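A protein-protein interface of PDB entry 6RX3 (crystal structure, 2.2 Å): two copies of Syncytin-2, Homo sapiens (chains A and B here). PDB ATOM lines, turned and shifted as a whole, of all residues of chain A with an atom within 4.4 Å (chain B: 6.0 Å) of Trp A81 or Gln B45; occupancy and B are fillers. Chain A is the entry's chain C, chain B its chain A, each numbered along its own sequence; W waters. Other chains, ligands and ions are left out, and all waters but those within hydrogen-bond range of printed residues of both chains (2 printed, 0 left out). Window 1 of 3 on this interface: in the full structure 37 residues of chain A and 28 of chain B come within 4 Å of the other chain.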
ATOM      1  N   GLN A  43      15.231  -5.555  15.979  1.00  0.00           N
ATOM      2  CA  GLN A  43      16.357  -5.447  16.895  1.00  0.00           C
ATOM      3  C   GLN A  43      16.576  -4.008  17.296  1.00  0.00           C
ATOM      4  O   GLN A  43      16.829  -3.754  18.472  1.00  0.00           O
ATOM      5  CB  GLN A  43      17.656  -6.073  16.361  1.00  0.00           C
ATOM      6  CG  GLN A  43      18.798  -6.091  17.416  1.00  0.00           C
ATOM      7  CD  GLN A  43      18.475  -6.921  18.642  1.00  0.00           C
ATOM      8  OE1 GLN A  43      17.911  -8.009  18.546  1.00  0.00           O
ATOM      9  NE2 GLN A  43      18.818  -6.425  19.828  1.00  0.00           N
ATOM     10  N   ILE A  46      14.020  -3.215  19.990  1.00  0.00           N
ATOM     11  CA  ILE A  46      14.406  -3.887  21.233  1.00  0.00           C
ATOM     12  C   ILE A  46      15.513  -3.080  21.923  1.00  0.00           C
ATOM     13  O   ILE A  46      15.372  -2.779  23.108  1.00  0.00           O
ATOM     14  CB  ILE A  46      14.788  -5.371  20.980  1.00  0.00           C
ATOM     15  CG1 ILE A  46      13.504  -6.189  20.687  1.00  0.00           C
ATOM     16  CG2 ILE A  46      15.616  -5.982  22.163  1.00  0.00           C
ATOM     17  CD1 ILE A  46      13.711  -7.611  20.104  1.00  0.00           C
ATOM     18  N   ASP A  47      16.565  -2.675  21.161  1.00  0.00           N
ATOM     19  CA  ASP A  47      17.684  -1.866  21.672  1.00  0.00           C
ATOM     20  C   ASP A  47      17.203  -0.528  22.218  1.00  0.00           C
ATOM     21  O   ASP A  47      17.667  -0.090  23.267  1.00  0.00           O
ATOM     22  CB  ASP A  47      18.746  -1.639  20.579  1.00  0.00           C
ATOM     23  CG  ASP A  47      19.500  -2.875  20.121  1.00  0.00           C
ATOM     24  OD1 ASP A  47      19.500  -3.891  20.866  1.00  0.00           O
ATOM     25  OD2 ASP A  47      20.124  -2.819  19.040  1.00  0.00           O
ATOM     26  N   ALA A  50      15.012  -1.139  25.462  1.00  0.00           N
ATOM     27  CA  ALA A  50      15.884  -1.533  26.551  1.00  0.00           C
ATOM     28  C   ALA A  50      16.520  -0.360  27.262  1.00  0.00           C
ATOM     29  O   ALA A  50      16.592  -0.391  28.494  1.00  0.00           O
ATOM     30  CB  ALA A  50      16.946  -2.489  26.053  1.00  0.00           C
ATOM     31  N   PHE A  80      17.879  -8.879  35.406  1.00  0.00           N
ATOM     32  CA  PHE A  80      18.838  -8.158  34.578  1.00  0.00           C
ATOM     33  C   PHE A  80      18.580  -8.437  33.105  1.00  0.00           C
ATOM     34  O   PHE A  80      18.245  -9.569  32.727  1.00  0.00           O
ATOM     35  CB  PHE A  80      20.263  -8.585  34.939  1.00  0.00           C
ATOM     36  CG  PHE A  80      20.711  -8.194  36.326  1.00  0.00           C
ATOM     37  CD1 PHE A  80      21.316  -6.968  36.558  1.00  0.00           C
ATOM     38  CD2 PHE A  80      20.530  -9.056  37.401  1.00  0.00           C
ATOM     39  CE1 PHE A  80      21.717  -6.602  37.845  1.00  0.00           C
ATOM     40  CE2 PHE A  80      20.946  -8.699  38.682  1.00  0.00           C
ATOM     41  CZ  PHE A  80      21.534  -7.474  38.897  1.00  0.00           C
ATOM     42  N   TRP A  81      18.718  -7.407  32.263  1.00  0.00           N
ATOM     43  CA  TRP A  81      18.528  -7.619  30.835  1.00  0.00           C
ATOM     44  C   TRP A  81      19.769  -8.235  30.201  1.00  0.00           C
ATOM     45  O   TRP A  81      20.889  -7.782  30.459  1.00  0.00           O
ATOM     46  CB  TRP A  81      18.098  -6.349  30.060  1.00  0.00           C
ATOM     47  CG  TRP A  81      17.749  -6.669  28.619  1.00  0.00           C
ATOM     48  CD1 TRP A  81      16.905  -7.651  28.176  1.00  0.00           C
ATOM     49  CD2 TRP A  81      18.318  -6.076  27.451  1.00  0.00           C
ATOM     50  NE1 TRP A  81      16.862  -7.660  26.800  1.00  0.00           N
ATOM     51  CE2 TRP A  81      17.727  -6.707  26.327  1.00  0.00           C
ATOM     52  CE3 TRP A  81      19.283  -5.080  27.243  1.00  0.00           C
ATOM     53  CZ2 TRP A  81      18.070  -6.374  25.020  1.00  0.00           C
ATOM     54  CZ3 TRP A  81      19.590  -4.719  25.941  1.00  0.00           C
ATOM     55  CH2 TRP A  81      18.993  -5.365  24.848  1.00  0.00           C
ATOM     56  N   VAL A  82      19.555  -9.241  29.347  1.00  0.00           N
ATOM     57  CA  VAL A  82      20.630  -9.898  28.628  1.00  0.00           C
ATOM     58  C   VAL A  82      20.589  -9.392  27.194  1.00  0.00           C
ATOM     59  O   VAL A  82      19.768  -9.817  26.377  1.00  0.00           O
ATOM     60  CB  VAL A  82      20.616 -11.448  28.787  1.00  0.00           C
ATOM     61  CG1 VAL A  82      21.675 -12.124  27.917  1.00  0.00           C
ATOM     62  CG2 VAL A  82      20.803 -11.833  30.245  1.00  0.00           C
ATOM     63  N   ASN A  83      21.461  -8.412  26.930  1.00  0.00           N
ATOM     64  CA  ASN A  83      21.651  -7.799  25.630  1.00  0.00           C
ATOM     65  C   ASN A  83      22.290  -8.832  24.705  1.00  0.00           C
ATOM     66  O   ASN A  83      23.347  -9.387  25.008  1.00  0.00           O
ATOM     67  CB  ASN A  83      22.535  -6.553  25.755  1.00  0.00           C
ATOM     68  CG  ASN A  83      22.620  -5.678  24.516  1.00  0.00           C
ATOM     69  OD1 ASN A  83      22.397  -6.097  23.374  1.00  0.00           O
ATOM     70  ND2 ASN A  83      23.016  -4.437  24.722  1.00  0.00           N
ATOM     71  N   GLN A  84      21.670  -9.081  23.563  1.00  0.00           N
ATOM     72  CA  GLN A  84      22.167 -10.034  22.582  1.00  0.00           C
ATOM     73  C   GLN A  84      22.101  -9.477  21.161  1.00  0.00           C
ATOM     74  O   GLN A  84      21.950 -10.216  20.195  1.00  0.00           O
ATOM     75  CB  GLN A  84      21.399 -11.339  22.675  1.00  0.00           C
ATOM     76  CG  GLN A  84      21.730 -12.201  23.878  1.00  0.00           C
ATOM     77  CD  GLN A  84      21.329 -13.647  23.671  1.00  0.00           C
ATOM     78  OE1 GLN A  84      22.087 -14.438  23.115  1.00  0.00           O
ATOM     79  NE2 GLN A  84      20.128 -13.997  24.111  1.00  0.00           N
ATOM     80  N   SER A  85      22.208  -8.156  21.068  1.00  0.00           N
ATOM     81  CA  SER A  85      22.151  -7.438  19.787  1.00  0.00           C
ATOM     82  C   SER A  85      23.221  -7.889  18.795  1.00  0.00           C
ATOM     83  O   SER A  85      22.916  -8.032  17.617  1.00  0.00           O
ATOM     84  CB  SER A  85      22.189  -5.926  19.987  1.00  0.00           C
ATOM     85  OG  SER A  85      23.397  -5.499  20.594  1.00  0.00           O
ATOM     86  N   VAL A  88      22.267 -11.248  17.080  1.00  0.00           N
ATOM     87  CA  VAL A  88      21.161 -11.021  16.131  1.00  0.00           C
ATOM     88  C   VAL A  88      21.696 -10.329  14.885  1.00  0.00           C
ATOM     89  O   VAL A  88      21.353 -10.737  13.791  1.00  0.00           O
ATOM     90  CB  VAL A  88      19.942 -10.296  16.773  1.00  0.00           C
ATOM     91  CG1 VAL A  88      18.998  -9.721  15.721  1.00  0.00           C
ATOM     92  CG2 VAL A  88      19.182 -11.230  17.695  1.00  0.00           C
ATOM     93  N   THR B  40      14.868 -17.174  17.822  1.00  0.00           N
ATOM     94  CA  THR B  40      15.138 -17.724  19.161  1.00  0.00           C
ATOM     95  C   THR B  40      15.843 -16.665  20.023  1.00  0.00           C
ATOM     96  O   THR B  40      15.417 -16.413  21.152  1.00  0.00           O
ATOM     97  CB  THR B  40      15.966 -19.035  19.060  1.00  0.00           C
ATOM     98  OG1 THR B  40      15.195 -20.038  18.399  1.00  0.00           O
ATOM     99  CG2 THR B  40      16.438 -19.558  20.419  1.00  0.00           C
ATOM    100  N   THR B  41      16.912 -16.052  19.477  1.00  0.00           N
ATOM    101  CA  THR B  41      17.697 -15.006  20.146  1.00  0.00           C
ATOM    102  C   THR B  41      16.834 -13.749  20.408  1.00  0.00           C
ATOM    103  O   THR B  41      16.920 -13.160  21.486  1.00  0.00           O
ATOM    104  CB  THR B  41      18.955 -14.711  19.328  1.00  0.00           C
ATOM    105  OG1 THR B  41      19.524 -15.953  18.922  1.00  0.00           O
ATOM    106  CG2 THR B  41      19.971 -13.875  20.095  1.00  0.00           C
ATOM    107  N   MET B  42      15.992 -13.376  19.432  1.00  0.00           N
ATOM    108  CA  MET B  42      15.070 -12.253  19.531  1.00  0.00           C
ATOM    109  C   MET B  42      14.042 -12.490  20.664  1.00  0.00           C
ATOM    110  O   MET B  42      13.835 -11.591  21.480  1.00  0.00           O
ATOM    111  CB  MET B  42      14.393 -12.013  18.179  1.00  0.00           C
ATOM    112  CG  MET B  42      13.832 -10.613  18.014  1.00  0.00           C
ATOM    113  SD  MET B  42      14.055 -10.016  16.319  1.00  0.00           S
ATOM    114  CE  MET B  42      15.541  -9.214  16.488  1.00  0.00           C
ATOM    115  N   GLN B  43      13.457 -13.719  20.746  1.00  0.00           N
ATOM    116  CA  GLN B  43      12.499 -14.080  21.802  1.00  0.00           C
ATOM    117  C   GLN B  43      13.155 -14.134  23.162  1.00  0.00           C
ATOM    118  O   GLN B  43      12.545 -13.693  24.122  1.00  0.00           O
ATOM    119  CB  GLN B  43      11.716 -15.379  21.484  1.00  0.00           C
ATOM    120  CG  GLN B  43      10.497 -15.634  22.412  1.00  0.00           C
ATOM    121  CD  GLN B  43       9.434 -14.554  22.390  1.00  0.00           C
ATOM    122  OE1 GLN B  43       8.931 -14.156  21.347  1.00  0.00           O
ATOM    123  NE2 GLN B  43       9.018 -14.088  23.556  1.00  0.00           N
ATOM    124  N   GLU B  44      14.410 -14.604  23.249  1.00  0.00           N
ATOM    125  CA  GLU B  44      15.165 -14.629  24.509  1.00  0.00           C
ATOM    126  C   GLU B  44      15.315 -13.215  25.084  1.00  0.00           C
ATOM    127  O   GLU B  44      15.114 -13.024  26.279  1.00  0.00           O
ATOM    128  CB  GLU B  44      16.549 -15.256  24.310  1.00  0.00           C
ATOM    129  CG  GLU B  44      16.542 -16.767  24.279  1.00  0.00           C
ATOM    130  CD  GLU B  44      17.820 -17.430  23.801  1.00  0.00           C
ATOM    131  OE1 GLU B  44      18.832 -16.727  23.573  1.00  0.00           O
ATOM    132  OE2 GLU B  44      17.798 -18.667  23.631  1.00  0.00           O
ATOM    133  N   GLN B  45      15.639 -12.227  24.212  1.00  0.00           N
ATOM    134  CA  GLN B  45      15.783 -10.812  24.567  1.00  0.00           C
ATOM    135  C   GLN B  45      14.466 -10.192  25.013  1.00  0.00           C
ATOM    136  O   GLN B  45      14.476  -9.405  25.943  1.00  0.00           O
ATOM    137  CB  GLN B  45      16.365 -10.009  23.406  1.00  0.00           C
ATOM    138  CG  GLN B  45      17.830 -10.267  23.162  1.00  0.00           C
ATOM    139  CD  GLN B  45      18.288  -9.521  21.943  1.00  0.00           C
ATOM    140  OE1 GLN B  45      18.990  -8.516  22.044  1.00  0.00           O
ATOM    141  NE2 GLN B  45      17.857  -9.973  20.771  1.00  0.00           N
ATOM    142  N   ILE B  46      13.350 -10.519  24.341  1.00  0.00           N
ATOM    143  CA  ILE B  46      12.006 -10.030  24.699  1.00  0.00           C
ATOM    144  C   ILE B  46      11.630 -10.561  26.091  1.00  0.00           C
ATOM    145  O   ILE B  46      11.190  -9.787  26.941  1.00  0.00           O
ATOM    146  CB  ILE B  46      10.964 -10.412  23.620  1.00  0.00           C
ATOM    147  CG1 ILE B  46      11.164  -9.542  22.359  1.00  0.00           C
ATOM    148  CG2 ILE B  46       9.508 -10.318  24.168  1.00  0.00           C
ATOM    149  CD1 ILE B  46      10.623 -10.067  21.118  1.00  0.00           C
ATOM    150  N   ASP B  47      11.823 -11.873  26.312  1.00  0.00           N
ATOM    151  CA  ASP B  47      11.551 -12.534  27.581  1.00  0.00           C
ATOM    152  C   ASP B  47      12.442 -11.962  28.685  1.00  0.00           C
ATOM    153  O   ASP B  47      11.954 -11.718  29.787  1.00  0.00           O
ATOM    154  CB  ASP B  47      11.708 -14.063  27.453  1.00  0.00           C
ATOM    155  CG  ASP B  47      10.712 -14.736  26.504  1.00  0.00           C
ATOM    156  OD1 ASP B  47       9.608 -14.169  26.287  1.00  0.00           O
ATOM    157  OD2 ASP B  47      11.043 -15.826  25.966  1.00  0.00           O
ATOM    158  N   SER B  48      13.738 -11.720  28.376  1.00  0.00           N
ATOM    159  CA  SER B  48      14.695 -11.146  29.315  1.00  0.00           C
ATOM    160  C   SER B  48      14.261  -9.728  29.698  1.00  0.00           C
ATOM    161  O   SER B  48      14.224  -9.404  30.889  1.00  0.00           O
ATOM    162  CB  SER B  48      16.106 -11.153  28.718  1.00  0.00           C
ATOM    163  OG  SER B  48      17.060 -10.579  29.595  1.00  0.00           O
ATOM    164  N   LEU B  49      13.916  -8.892  28.687  1.00  0.00           N
ATOM    165  CA  LEU B  49      13.475  -7.521  28.894  1.00  0.00           C
ATOM    166  C   LEU B  49      12.159  -7.435  29.656  1.00  0.00           C
ATOM    167  O   LEU B  49      12.048  -6.611  30.563  1.00  0.00           O
ATOM    168  CB  LEU B  49      13.423  -6.718  27.566  1.00  0.00           C
ATOM    169  CG  LEU B  49      13.383  -5.189  27.718  1.00  0.00           C
ATOM    170  CD1 LEU B  49      14.665  -4.642  28.393  1.00  0.00           C
ATOM    171  CD2 LEU B  49      13.125  -4.506  26.370  1.00  0.00           C
ATOM    172  N   ALA B  50      11.180  -8.292  29.318  1.00  0.00           N
ATOM    173  CA  ALA B  50       9.878  -8.308  29.986  1.00  0.00           C
ATOM    174  C   ALA B  50       9.961  -8.611  31.472  1.00  0.00           C
ATOM    175  O   ALA B  50       9.237  -7.983  32.234  1.00  0.00           O
ATOM    176  CB  ALA B  50       8.944  -9.277  29.303  1.00  0.00           C
ATOM    177  N   VAL B  52      12.347  -7.686  33.456  1.00  0.00           N
ATOM    178  CA  VAL B  52      12.853  -6.428  34.028  1.00  0.00           C
ATOM    179  C   VAL B  52      11.716  -5.397  34.110  1.00  0.00           C
ATOM    180  O   VAL B  52      11.553  -4.775  35.159  1.00  0.00           O
ATOM    181  CB  VAL B  52      14.110  -5.876  33.281  1.00  0.00           C
ATOM    182  CG1 VAL B  52      14.634  -4.592  33.945  1.00  0.00           C
ATOM    183  CG2 VAL B  52      15.203  -6.926  33.215  1.00  0.00           C
HETATM  184  O   HOH W   1      15.505 -10.436  33.058  1.00  0.00           O
HETATM  185  O   HOH W   2      18.542 -12.268  25.902  1.00  0.00           O
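The backbone carbonyl oxygen of Thr B41 sits at hydrogen-bond distance from the side-chain amide nitrogen of Gln B45 (3.4 Å).
OD1 of Asn A83 lies within hydrogen-bond range of OG of Ser A85 (3.0 Å).
The side-chain amide nitrogen (NE2) of Gln A43 is in hydrogen-bond range of the side-chain carboxylate (OD1) of Asp A47 (2.8 Å).
Water W1 lies within hydrogen-bond range of O of Ser B48 (2.7 Å) and O of Phe A80 (2.9 Å).
Water W2 lies within hydrogen-bond range of O of Val A82, NE2 of Gln A84 and N of Gln B45.
Ile B46 touches its own counterpart, Ile A46.
Positions printed for both chains: 43, 46, 47 and 50.
Of the 20 pairs that touch across the chains among the printed residues, 1 has its exchanged pair printed and touching as well.
Trp A81 touches just these residues of chain B: Gln B45 (3.1 Å), Ser B48 (3.3 Å), Leu B49 (3.3 Å) and Val B52 (3.7 Å).
Gln B45 touches just these residues of chain A: Gln A43 (3.0 Å), Trp A81 (3.1 Å), Val A82 (3.8 Å), Gln A84 (3.1 Å), Ser A85 (3.4 Å) and Val A88 (3.6 Å).
Of the printed residues of chain A, Glu B44 touches Gln A84 (3.1 Å).
Of the printed residues of chain A, Leu B49 touches Ala A50 and Trp A81.
Asn A83 touches none of the printed residues of chain B.
Thr B40 touches none of the printed residues of chain A.
The nearest residue of chain B that does not touch Trp A81 is Ile B46 (5.2 Å).
Met B42 touches Gln A43.
Ile A46 touches Met B42.
Ile B46 touches Ile A46.
CD1 of Leu B49 touches CA of Ala A50 (3.8 Å).
CG2 of Val B52 touches C of Phe A80, 3.7 Å away.
Trp A81 touches Ser B48.
O of Val A82 touches CG of Gln B45, at 3.8 Å.
Thr B41 touches Gln A84.
Val A88 touches Thr B41.
Val A88 touches Met B42 (CG1 to CE, 3.6 Å).
Of the 12 printed residues of chain B, 8 touch a printed residue of chain A.
Hydrophobic or aromatic side chains of chain B within 4 Å of the printed part of chain A: Met B42, Ile B46, Leu B49 and Val B52.
Printed residues of chain A that touch a printed residue of chain B: Gln A43, Ile A46, Ala A50, Phe A80, Trp A81, Val A82, Gln A84, Ser A85 and Val A88.
Hydrophobic or aromatic side chains of chain A that line the printed part of chain B: Ile A46, Ala A50, Trp A81, Val A82 and Val A88.
Among the printed residues, no Asp or Glu carboxylate lies within 4 Å of a Lys or Arg side-chain nitrogen of the other chain.
The backbone carbonyl oxygen (O) of Phe A80 lies within hydrogen-bond range of the side-chain hydroxyl (OG) of Ser B48 (3.5 Å).
The backbone NH of Gln A84 is in hydrogen-bond range of the side-chain amide oxygen of Gln B45, 3.1 Å away.
The side-chain hydroxyl (OG) of Ser B48 lies within hydrogen-bond range of the backbone NH (N) of Val A82 (2.8 Å).
NE1 of Trp A81 lies within hydrogen-bond range of O of Gln B45.
The side-chain carboxylate of Glu B44 lies within hydrogen-bond range of the side-chain amide nitrogen of Gln A84, at 3.1 Å.
The side-chain amide oxygen (OE1) of Gln B45 sits at hydrogen-bond distance from the backbone NH (N) of Ser A85.
The side-chain amide oxygen (OE1) of Gln A43 sits at hydrogen-bond distance from the side-chain amide nitrogen (NE2) of Gln B45.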
